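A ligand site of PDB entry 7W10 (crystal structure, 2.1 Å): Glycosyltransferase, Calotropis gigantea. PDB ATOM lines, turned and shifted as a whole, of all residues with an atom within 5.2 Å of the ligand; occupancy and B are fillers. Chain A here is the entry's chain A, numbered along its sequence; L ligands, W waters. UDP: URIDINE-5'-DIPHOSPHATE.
N of Gly 285 sits at hydrogen-bond distance from OG of Ser 283, at 3.2 Å.
O of Gly 26 lies within hydrogen-bond range of ND2 of Asn 375 (2.5 Å).
The side-chain carboxylate of Glu 379 sits close to the side-chain amide oxygen of Gln 356.
A ring nitrogen (ND1) of His 371 lies close to the backbone NH (N) of Gly 373 (3.4 Å).
The backbone carbonyl oxygen of Gly 373 is in hydrogen-bond range of the side-chain hydroxyl of Thr 377, 3.0 Å away.
The indole nitrogen of Trp 353 lies within hydrogen-bond range of the side-chain carboxylate of Glu 261 (3.0 Å).
The side-chain hydroxyl of Tyr 281 sits at hydrogen-bond distance from the side-chain amide nitrogen of Gln 356 (2.7 Å).
The side-chain hydroxyl (OH) of Tyr 281 is in hydrogen-bond range of the side-chain sulfur (SG) of Cys 354 (3.1 Å).
SG of Cys 354 lies within hydrogen-bond range of O4 of the ligand (3.4 Å).
The side-chain hydroxyl of Ser 286 is in hydrogen-bond range of an oxygen (O2B) of the ligand, 2.7 Å away.
The side-chain amide nitrogen (ND2) of Asn 29 is in hydrogen-bond range of an oxygen (O3') of the ligand (2.9 Å).
The backbone NH of Ser 376 is in hydrogen-bond range of an oxygen (O1A) of the ligand.
N of Asn 375 lies close to O2A of the ligand (3.3 Å).
N3 of the ligand is in hydrogen-bond range of O of Cys 354, at 2.6 Å.
The backbone NH (N) of Cys 354 sits at hydrogen-bond distance from an oxygen (O4) of the ligand, at 3.2 Å.
ND2 of Asn 375 lies within hydrogen-bond range of O2A of the ligand (2.9 Å).
The side-chain carboxylate (OE1) of Glu 379 is in hydrogen-bond range of an oxygen (O2') of the ligand, at 2.7 Å.
An oxygen (O3A) of the ligand lies within hydrogen-bond range of a ring nitrogen (NE2) of His 371, 2.9 Å away.
The backbone NH (N) of Ser 286 sits at hydrogen-bond distance from an oxygen (O2B) of the ligand (2.7 Å).
The side-chain hydroxyl of Ser 376 is in hydrogen-bond range of an oxygen (O1A) of the ligand (2.6 Å).
O2 of the ligand sits close to OE2 of Glu 261 (2.9 Å).
Gly 26 touches the ligand (CA to C5', 3.5 Å).
OH of Tyr 281 touches O4 of the ligand, 3.7 Å away.
Ser 283 touches the ligand.
C of Gly 285 touches O2B of the ligand, 3.7 Å away.
N of Ile 287 touches O2B of the ligand, 3.99 Å away.
CG1 of Val 312 touches O4 of the ligand, 3.4 Å away.
CZ2 of Trp 353 touches C2 of the ligand, 3.2 Å away.
Gln 356 touches the ligand.
CA of Gly 373 touches O1A of the ligand (3.5 Å).
Hydrophobic or aromatic side chains that line the ligand: Val 312, Trp 353 and His 371.
Of the 26 residues printed, 17 come within 4 Å of the ligand.
The nearest printed residue that does not touch the ligand is Trp 374 (4.02 Å).
Water W1 lies within hydrogen-bond range of NE2 of Gln 356, OG of Ser 283 and OG of Ser 376.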
ATOM      1  N   LYS A  25      17.795 -19.431  -4.571  1.00  0.00           N
ATOM      2  CA  LYS A  25      18.567 -20.015  -3.471  1.00  0.00           C
ATOM      3  C   LYS A  25      18.419 -19.233  -2.182  1.00  0.00           C
ATOM      4  O   LYS A  25      18.454 -19.822  -1.096  1.00  0.00           O
ATOM      5  CB  LYS A  25      20.046 -20.141  -3.849  1.00  0.00           C
ATOM      6  CG  LYS A  25      20.394 -21.498  -4.459  1.00  0.00           C
ATOM      7  CD  LYS A  25      21.254 -21.333  -5.683  1.00  0.00           C
ATOM      8  CE  LYS A  25      22.234 -22.464  -5.859  1.00  0.00           C
ATOM      9  NZ  LYS A  25      22.856 -22.399  -7.209  1.00  0.00           N
ATOM     10  N   GLY A  26      18.235 -17.912  -2.283  1.00  0.00           N
ATOM     11  CA  GLY A  26      18.017 -17.101  -1.106  1.00  0.00           C
ATOM     12  C   GLY A  26      16.683 -17.356  -0.428  1.00  0.00           C
ATOM     13  O   GLY A  26      16.491 -16.938   0.724  1.00  0.00           O
ATOM     14  N   ASN A  29      17.053 -21.869   0.561  1.00  0.00           N
ATOM     15  CA  ASN A  29      17.940 -22.259   1.658  1.00  0.00           C
ATOM     16  C   ASN A  29      17.296 -22.031   3.009  1.00  0.00           C
ATOM     17  O   ASN A  29      17.265 -22.975   3.814  1.00  0.00           O
ATOM     18  CB  ASN A  29      19.280 -21.528   1.545  1.00  0.00           C
ATOM     19  CG  ASN A  29      20.248 -22.192   0.570  1.00  0.00           C
ATOM     20  OD1 ASN A  29      19.952 -23.235  -0.052  1.00  0.00           O
ATOM     21  ND2 ASN A  29      21.410 -21.562   0.392  1.00  0.00           N
ATOM     22  N   GLU A 261      26.606 -28.352   0.365  1.00  0.00           N
ATOM     23  CA  GLU A 261      26.852 -27.491  -0.782  1.00  0.00           C
ATOM     24  C   GLU A 261      28.056 -27.988  -1.590  1.00  0.00           C
ATOM     25  O   GLU A 261      28.840 -28.829  -1.145  1.00  0.00           O
ATOM     26  CB  GLU A 261      27.086 -26.044  -0.342  1.00  0.00           C
ATOM     27  CG  GLU A 261      25.864 -25.331   0.246  1.00  0.00           C
ATOM     28  CD  GLU A 261      25.010 -24.663  -0.808  1.00  0.00           C
ATOM     29  OE1 GLU A 261      25.144 -25.029  -1.996  1.00  0.00           O
ATOM     30  OE2 GLU A 261      24.201 -23.763  -0.458  1.00  0.00           O
ATOM     31  N   TYR A 281      36.818 -13.371   2.901  1.00  0.00           N
ATOM     32  CA  TYR A 281      35.855 -14.137   2.122  1.00  0.00           C
ATOM     33  C   TYR A 281      34.953 -13.168   1.371  1.00  0.00           C
ATOM     34  O   TYR A 281      34.348 -12.269   1.972  1.00  0.00           O
ATOM     35  CB  TYR A 281      35.043 -15.082   3.033  1.00  0.00           C
ATOM     36  CG  TYR A 281      33.846 -15.728   2.336  1.00  0.00           C
ATOM     37  CD1 TYR A 281      34.021 -16.491   1.178  1.00  0.00           C
ATOM     38  CD2 TYR A 281      32.553 -15.560   2.832  1.00  0.00           C
ATOM     39  CE1 TYR A 281      32.934 -17.074   0.535  1.00  0.00           C
ATOM     40  CE2 TYR A 281      31.454 -16.116   2.183  1.00  0.00           C
ATOM     41  CZ  TYR A 281      31.651 -16.897   1.041  1.00  0.00           C
ATOM     42  OH  TYR A 281      30.565 -17.454   0.411  1.00  0.00           O
ATOM     43  N   SER A 283      31.846 -12.719  -1.518  1.00  0.00           N
ATOM     44  CA  SER A 283      30.792 -13.342  -2.306  1.00  0.00           C
ATOM     45  C   SER A 283      29.651 -12.363  -2.505  1.00  0.00           C
ATOM     46  O   SER A 283      29.250 -11.642  -1.588  1.00  0.00           O
ATOM     47  CB  SER A 283      30.264 -14.626  -1.629  1.00  0.00           C
ATOM     48  OG  SER A 283      29.100 -15.068  -2.308  1.00  0.00           O
ATOM     49  N   PHE A 284      29.098 -12.351  -3.716  1.00  0.00           N
ATOM     50  CA  PHE A 284      27.979 -11.474  -4.013  1.00  0.00           C
ATOM     51  C   PHE A 284      26.695 -12.279  -4.231  1.00  0.00           C
ATOM     52  O   PHE A 284      25.777 -11.826  -4.900  1.00  0.00           O
ATOM     53  CB  PHE A 284      28.317 -10.588  -5.203  1.00  0.00           C
ATOM     54  CG  PHE A 284      29.319  -9.517  -4.859  1.00  0.00           C
ATOM     55  CD1 PHE A 284      30.673  -9.824  -4.786  1.00  0.00           C
ATOM     56  CD2 PHE A 284      28.913  -8.220  -4.562  1.00  0.00           C
ATOM     57  CE1 PHE A 284      31.611  -8.849  -4.450  1.00  0.00           C
ATOM     58  CE2 PHE A 284      29.848  -7.241  -4.217  1.00  0.00           C
ATOM     59  CZ  PHE A 284      31.197  -7.570  -4.149  1.00  0.00           C
ATOM     60  N   GLY A 285      26.621 -13.452  -3.612  1.00  0.00           N
ATOM     61  CA  GLY A 285      25.386 -14.211  -3.594  1.00  0.00           C
ATOM     62  C   GLY A 285      25.183 -14.976  -4.887  1.00  0.00           C
ATOM     63  O   GLY A 285      26.108 -15.159  -5.695  1.00  0.00           O
ATOM     64  N   SER A 286      23.940 -15.403  -5.103  1.00  0.00           N
ATOM     65  CA  SER A 286      23.593 -16.307  -6.183  1.00  0.00           C
ATOM     66  C   SER A 286      22.989 -15.619  -7.411  1.00  0.00           C
ATOM     67  O   SER A 286      22.939 -16.240  -8.469  1.00  0.00           O
ATOM     68  CB  SER A 286      22.612 -17.386  -5.683  1.00  0.00           C
ATOM     69  OG  SER A 286      21.343 -16.843  -5.367  1.00  0.00           O
ATOM     70  N   ILE A 287      22.568 -14.354  -7.318  1.00  0.00           N
ATOM     71  CA  ILE A 287      21.836 -13.680  -8.394  1.00  0.00           C
ATOM     72  C   ILE A 287      22.562 -12.442  -8.920  1.00  0.00           C
ATOM     73  O   ILE A 287      22.506 -12.155 -10.126  1.00  0.00           O
ATOM     74  CB  ILE A 287      20.404 -13.294  -7.925  1.00  0.00           C
ATOM     75  CG1 ILE A 287      19.562 -14.536  -7.680  1.00  0.00           C
ATOM     76  CG2 ILE A 287      19.739 -12.409  -8.973  1.00  0.00           C
ATOM     77  CD1 ILE A 287      18.280 -14.253  -6.926  1.00  0.00           C
ATOM     78  N   ALA A 288      23.231 -11.685  -8.049  1.00  0.00           N
ATOM     79  CA  ALA A 288      23.769 -10.380  -8.438  1.00  0.00           C
ATOM     80  C   ALA A 288      24.923 -10.526  -9.435  1.00  0.00           C
ATOM     81  O   ALA A 288      25.741 -11.448  -9.350  1.00  0.00           O
ATOM     82  CB  ALA A 288      24.252  -9.605  -7.208  1.00  0.00           C
ATOM     83  N   VAL A 312      34.226 -16.098  -4.362  1.00  0.00           N
ATOM     84  CA  VAL A 312      33.268 -16.855  -5.143  1.00  0.00           C
ATOM     85  C   VAL A 312      32.852 -16.010  -6.338  1.00  0.00           C
ATOM     86  O   VAL A 312      32.300 -14.915  -6.177  1.00  0.00           O
ATOM     87  CB  VAL A 312      32.044 -17.280  -4.297  1.00  0.00           C
ATOM     88  CG1 VAL A 312      31.186 -18.225  -5.093  1.00  0.00           C
ATOM     89  CG2 VAL A 312      32.490 -18.000  -3.039  1.00  0.00           C
ATOM     90  N   TRP A 353      31.837 -21.707  -6.390  1.00  0.00           N
ATOM     91  CA  TRP A 353      30.842 -21.904  -5.326  1.00  0.00           C
ATOM     92  C   TRP A 353      31.501 -22.519  -4.108  1.00  0.00           C
ATOM     93  O   TRP A 353      32.441 -23.325  -4.234  1.00  0.00           O
ATOM     94  CB  TRP A 353      29.683 -22.795  -5.793  1.00  0.00           C
ATOM     95  CG  TRP A 353      28.442 -22.654  -4.982  1.00  0.00           C
ATOM     96  CD1 TRP A 353      27.905 -23.589  -4.147  1.00  0.00           C
ATOM     97  CD2 TRP A 353      27.583 -21.508  -4.926  1.00  0.00           C
ATOM     98  NE1 TRP A 353      26.759 -23.097  -3.570  1.00  0.00           N
ATOM     99  CE2 TRP A 353      26.536 -21.824  -4.030  1.00  0.00           C
ATOM    100  CE3 TRP A 353      27.595 -20.244  -5.530  1.00  0.00           C
ATOM    101  CZ2 TRP A 353      25.512 -20.928  -3.745  1.00  0.00           C
ATOM    102  CZ3 TRP A 353      26.583 -19.363  -5.233  1.00  0.00           C
ATOM    103  CH2 TRP A 353      25.556 -19.701  -4.343  1.00  0.00           C
ATOM    104  N   CYS A 354      30.957 -22.177  -2.930  1.00  0.00           N
ATOM    105  CA  CYS A 354      31.480 -22.707  -1.677  1.00  0.00           C
ATOM    106  C   CYS A 354      30.377 -23.037  -0.669  1.00  0.00           C
ATOM    107  O   CYS A 354      29.226 -22.599  -0.832  1.00  0.00           O
ATOM    108  CB  CYS A 354      32.445 -21.697  -1.052  1.00  0.00           C
ATOM    109  SG  CYS A 354      31.593 -20.330  -0.224  1.00  0.00           S
ATOM    110  N   PRO A 355      30.668 -23.792   0.375  1.00  0.00           N
ATOM    111  CA  PRO A 355      29.700 -23.939   1.463  1.00  0.00           C
ATOM    112  C   PRO A 355      29.738 -22.708   2.351  1.00  0.00           C
ATOM    113  O   PRO A 355      30.593 -22.633   3.251  1.00  0.00           O
ATOM    114  CB  PRO A 355      30.177 -25.198   2.200  1.00  0.00           C
ATOM    115  CG  PRO A 355      31.677 -25.184   2.015  1.00  0.00           C
ATOM    116  CD  PRO A 355      31.952 -24.451   0.680  1.00  0.00           C
ATOM    117  N   GLN A 356      28.859 -21.732   2.134  1.00  0.00           N
ATOM    118  CA  GLN A 356      29.058 -20.426   2.762  1.00  0.00           C
ATOM    119  C   GLN A 356      29.040 -20.531   4.290  1.00  0.00           C
ATOM    120  O   GLN A 356      29.904 -19.947   4.968  1.00  0.00           O
ATOM    121  CB  GLN A 356      28.015 -19.434   2.294  1.00  0.00           C
ATOM    122  CG  GLN A 356      28.126 -18.118   3.021  1.00  0.00           C
ATOM    123  CD  GLN A 356      27.503 -16.997   2.226  1.00  0.00           C
ATOM    124  OE1 GLN A 356      26.486 -16.416   2.630  1.00  0.00           O
ATOM    125  NE2 GLN A 356      28.097 -16.696   1.088  1.00  0.00           N
ATOM    126  N   LEU A 357      28.062 -21.244   4.852  1.00  0.00           N
ATOM    127  CA  LEU A 357      27.976 -21.290   6.302  1.00  0.00           C
ATOM    128  C   LEU A 357      29.242 -21.917   6.890  1.00  0.00           C
ATOM    129  O   LEU A 357      29.788 -21.422   7.884  1.00  0.00           O
ATOM    130  CB  LEU A 357      26.718 -22.035   6.749  1.00  0.00           C
ATOM    131  CG  LEU A 357      26.205 -21.707   8.158  1.00  0.00           C
ATOM    132  CD1 LEU A 357      25.953 -20.210   8.324  1.00  0.00           C
ATOM    133  CD2 LEU A 357      24.949 -22.499   8.509  1.00  0.00           C
ATOM    134  N   HIS A 371      27.380  -8.750  -0.622  1.00  0.00           N
ATOM    135  CA  HIS A 371      26.314  -7.904  -1.177  1.00  0.00           C
ATOM    136  C   HIS A 371      25.178  -7.644  -0.187  1.00  0.00           C
ATOM    137  O   HIS A 371      24.234  -6.916  -0.521  1.00  0.00           O
ATOM    138  CB  HIS A 371      25.738  -8.533  -2.452  1.00  0.00           C
ATOM    139  CG  HIS A 371      24.813  -9.687  -2.200  1.00  0.00           C
ATOM    140  ND1 HIS A 371      25.114 -10.705  -1.328  1.00  0.00           N
ATOM    141  CD2 HIS A 371      23.603  -9.980  -2.731  1.00  0.00           C
ATOM    142  CE1 HIS A 371      24.125 -11.585  -1.329  1.00  0.00           C
ATOM    143  NE2 HIS A 371      23.182 -11.173  -2.167  1.00  0.00           N
ATOM    144  N   GLY A 373      22.798  -9.599   0.970  1.00  0.00           N
ATOM    145  CA  GLY A 373      21.583 -10.392   0.976  1.00  0.00           C
ATOM    146  C   GLY A 373      21.238 -10.820   2.404  1.00  0.00           C
ATOM    147  O   GLY A 373      22.160 -11.005   3.202  1.00  0.00           O
ATOM    148  N   TRP A 374      19.967 -10.995   2.745  1.00  0.00           N
ATOM    149  CA  TRP A 374      19.612 -11.255   4.141  1.00  0.00           C
ATOM    150  C   TRP A 374      20.187 -12.571   4.651  1.00  0.00           C
ATOM    151  O   TRP A 374      20.650 -12.647   5.794  1.00  0.00           O
ATOM    152  CB  TRP A 374      18.101 -11.238   4.343  1.00  0.00           C
ATOM    153  CG  TRP A 374      17.734 -11.486   5.811  1.00  0.00           C
ATOM    154  CD1 TRP A 374      16.934 -12.472   6.299  1.00  0.00           C
ATOM    155  CD2 TRP A 374      18.191 -10.721   6.952  1.00  0.00           C
ATOM    156  NE1 TRP A 374      16.856 -12.370   7.675  1.00  0.00           N
ATOM    157  CE2 TRP A 374      17.616 -11.312   8.099  1.00  0.00           C
ATOM    158  CE3 TRP A 374      19.018  -9.588   7.113  1.00  0.00           C
ATOM    159  CZ2 TRP A 374      17.841 -10.821   9.382  1.00  0.00           C
ATOM    160  CZ3 TRP A 374      19.254  -9.117   8.386  1.00  0.00           C
ATOM    161  CH2 TRP A 374      18.657  -9.736   9.513  1.00  0.00           C
ATOM    162  N   ASN A 375      20.160 -13.621   3.829  1.00  0.00           N
ATOM    163  CA  ASN A 375      20.733 -14.898   4.262  1.00  0.00           C
ATOM    164  C   ASN A 375      22.220 -14.750   4.598  1.00  0.00           C
ATOM    165  O   ASN A 375      22.678 -15.220   5.645  1.00  0.00           O
ATOM    166  CB  ASN A 375      20.521 -15.976   3.198  1.00  0.00           C
ATOM    167  CG  ASN A 375      19.080 -16.384   3.090  1.00  0.00           C
ATOM    168  OD1 ASN A 375      18.510 -16.921   4.050  1.00  0.00           O
ATOM    169  ND2 ASN A 375      18.466 -16.112   1.949  1.00  0.00           N
ATOM    170  N   SER A 376      22.972 -14.102   3.701  1.00  0.00           N
ATOM    171  CA  SER A 376      24.399 -13.883   3.933  1.00  0.00           C
ATOM    172  C   SER A 376      24.642 -13.027   5.168  1.00  0.00           C
ATOM    173  O   SER A 376      25.557 -13.292   5.951  1.00  0.00           O
ATOM    174  CB  SER A 376      25.044 -13.233   2.697  1.00  0.00           C
ATOM    175  OG  SER A 376      25.025 -14.144   1.628  1.00  0.00           O
ATOM    176  N   THR A 377      23.813 -12.005   5.373  1.00  0.00           N
ATOM    177  CA  THR A 377      23.923 -11.174   6.574  1.00  0.00           C
ATOM    178  C   THR A 377      23.647 -11.983   7.825  1.00  0.00           C
ATOM    179  O   THR A 377      24.442 -11.977   8.790  1.00  0.00           O
ATOM    180  CB  THR A 377      22.947  -9.978   6.465  1.00  0.00           C
ATOM    181  OG1 THR A 377      23.256  -9.195   5.309  1.00  0.00           O
ATOM    182  CG2 THR A 377      23.036  -9.063   7.690  1.00  0.00           C
ATOM    183  N   GLU A 379      23.629 -15.254   8.228  1.00  0.00           N
ATOM    184  CA  GLU A 379      24.678 -16.251   8.409  1.00  0.00           C
ATOM    185  C   GLU A 379      25.943 -15.639   9.009  1.00  0.00           C
ATOM    186  O   GLU A 379      26.596 -16.250   9.860  1.00  0.00           O
ATOM    187  CB  GLU A 379      24.994 -16.932   7.074  1.00  0.00           C
ATOM    188  CG  GLU A 379      23.917 -17.917   6.660  1.00  0.00           C
ATOM    189  CD  GLU A 379      24.004 -18.317   5.198  1.00  0.00           C
ATOM    190  OE1 GLU A 379      24.993 -17.963   4.531  1.00  0.00           O
ATOM    191  OE2 GLU A 379      23.085 -18.999   4.705  1.00  0.00           O
ATOM    192  N   TRP A 393      21.010  -4.189  -4.518  1.00  0.00           N
ATOM    193  CA  TRP A 393      19.644  -3.774  -4.820  1.00  0.00           C
ATOM    194  C   TRP A 393      18.669  -4.382  -3.822  1.00  0.00           C
ATOM    195  O   TRP A 393      19.042  -5.217  -2.990  1.00  0.00           O
ATOM    196  CB  TRP A 393      19.251  -4.132  -6.256  1.00  0.00           C
ATOM    197  CG  TRP A 393      19.904  -5.356  -6.797  1.00  0.00           C
ATOM    198  CD1 TRP A 393      20.928  -5.412  -7.725  1.00  0.00           C
ATOM    199  CD2 TRP A 393      19.573  -6.711  -6.487  1.00  0.00           C
ATOM    200  NE1 TRP A 393      21.249  -6.729  -7.990  1.00  0.00           N
ATOM    201  CE2 TRP A 393      20.433  -7.542  -7.245  1.00  0.00           C
ATOM    202  CE3 TRP A 393      18.628  -7.301  -5.637  1.00  0.00           C
ATOM    203  CZ2 TRP A 393      20.368  -8.945  -7.176  1.00  0.00           C
ATOM    204  CZ3 TRP A 393      18.571  -8.687  -5.573  1.00  0.00           C
ATOM    205  CH2 TRP A 393      19.444  -9.492  -6.337  1.00  0.00           C
ATOM    206  N   GLN A 396      19.215  -5.092   0.169  1.00  0.00           N
ATOM    207  CA  GLN A 396      20.638  -5.073   0.501  1.00  0.00           C
ATOM    208  C   GLN A 396      21.090  -3.704   0.997  1.00  0.00           C
ATOM    209  O   GLN A 396      21.976  -3.628   1.864  1.00  0.00           O
ATOM    210  CB  GLN A 396      21.465  -5.531  -0.694  1.00  0.00           C
ATOM    211  CG  GLN A 396      21.124  -6.986  -1.141  1.00  0.00           C
ATOM    212  CD  GLN A 396      21.431  -7.250  -2.594  1.00  0.00           C
ATOM    213  OE1 GLN A 396      22.217  -6.534  -3.238  1.00  0.00           O
ATOM    214  NE2 GLN A 396      20.792  -8.293  -3.138  1.00  0.00           N
HETATM  215  N1  UDP L   1      25.533 -19.278  -0.812  1.00  0.00           N
HETATM  216  C2  UDP L   1      26.347 -20.535  -0.708  1.00  0.00           C
HETATM  217  N3  UDP L   1      27.718 -20.578  -1.332  1.00  0.00           N
HETATM  218  C4  UDP L   1      28.247 -19.402  -2.031  1.00  0.00           C
HETATM  219  C5  UDP L   1      27.428 -18.154  -2.133  1.00  0.00           C
HETATM  220  C6  UDP L   1      26.065 -18.126  -1.511  1.00  0.00           C
HETATM  221  O2  UDP L   1      25.929 -21.487  -0.133  1.00  0.00           O
HETATM  222  O4  UDP L   1      29.326 -19.423  -2.529  1.00  0.00           O
HETATM  223  C1' UDP L   1      24.180 -19.233  -0.240  1.00  0.00           C
HETATM  224  C2' UDP L   1      24.087 -18.497   1.199  1.00  0.00           C
HETATM  225  O2' UDP L   1      24.625 -19.381   2.239  1.00  0.00           O
HETATM  226  C3' UDP L   1      22.801 -18.240   1.376  1.00  0.00           C
HETATM  227  C4' UDP L   1      22.160 -18.246  -0.027  1.00  0.00           C
HETATM  228  O4' UDP L   1      23.336 -18.565  -0.997  1.00  0.00           O
HETATM  229  O3' UDP L   1      22.140 -19.344   2.163  1.00  0.00           O
HETATM  230  C5' UDP L   1      21.409 -17.063  -0.306  1.00  0.00           C
HETATM  231  O5' UDP L   1      22.134 -15.905  -0.563  1.00  0.00           O
HETATM  232  PA  UDP L   1      21.627 -14.385  -0.103  1.00  0.00           P
HETATM  233  O1A UDP L   1      22.654 -13.727   0.774  1.00  0.00           O
HETATM  234  O2A UDP L   1      20.296 -14.367   0.583  1.00  0.00           O
HETATM  235  O3A UDP L   1      21.467 -13.418  -1.421  1.00  0.00           O
HETATM  236  PB  UDP L   1      20.962 -13.885  -2.915  1.00  0.00           P
HETATM  237  O1B UDP L   1      21.158 -12.659  -3.822  1.00  0.00           O
HETATM  238  O2B UDP L   1      21.792 -15.026  -3.465  1.00  0.00           O
HETATM  239  O3B UDP L   1      19.493 -14.281  -2.840  1.00  0.00           O
HETATM  240  O   HOH W   1      26.846 -15.083  -0.483  1.00  0.00           O
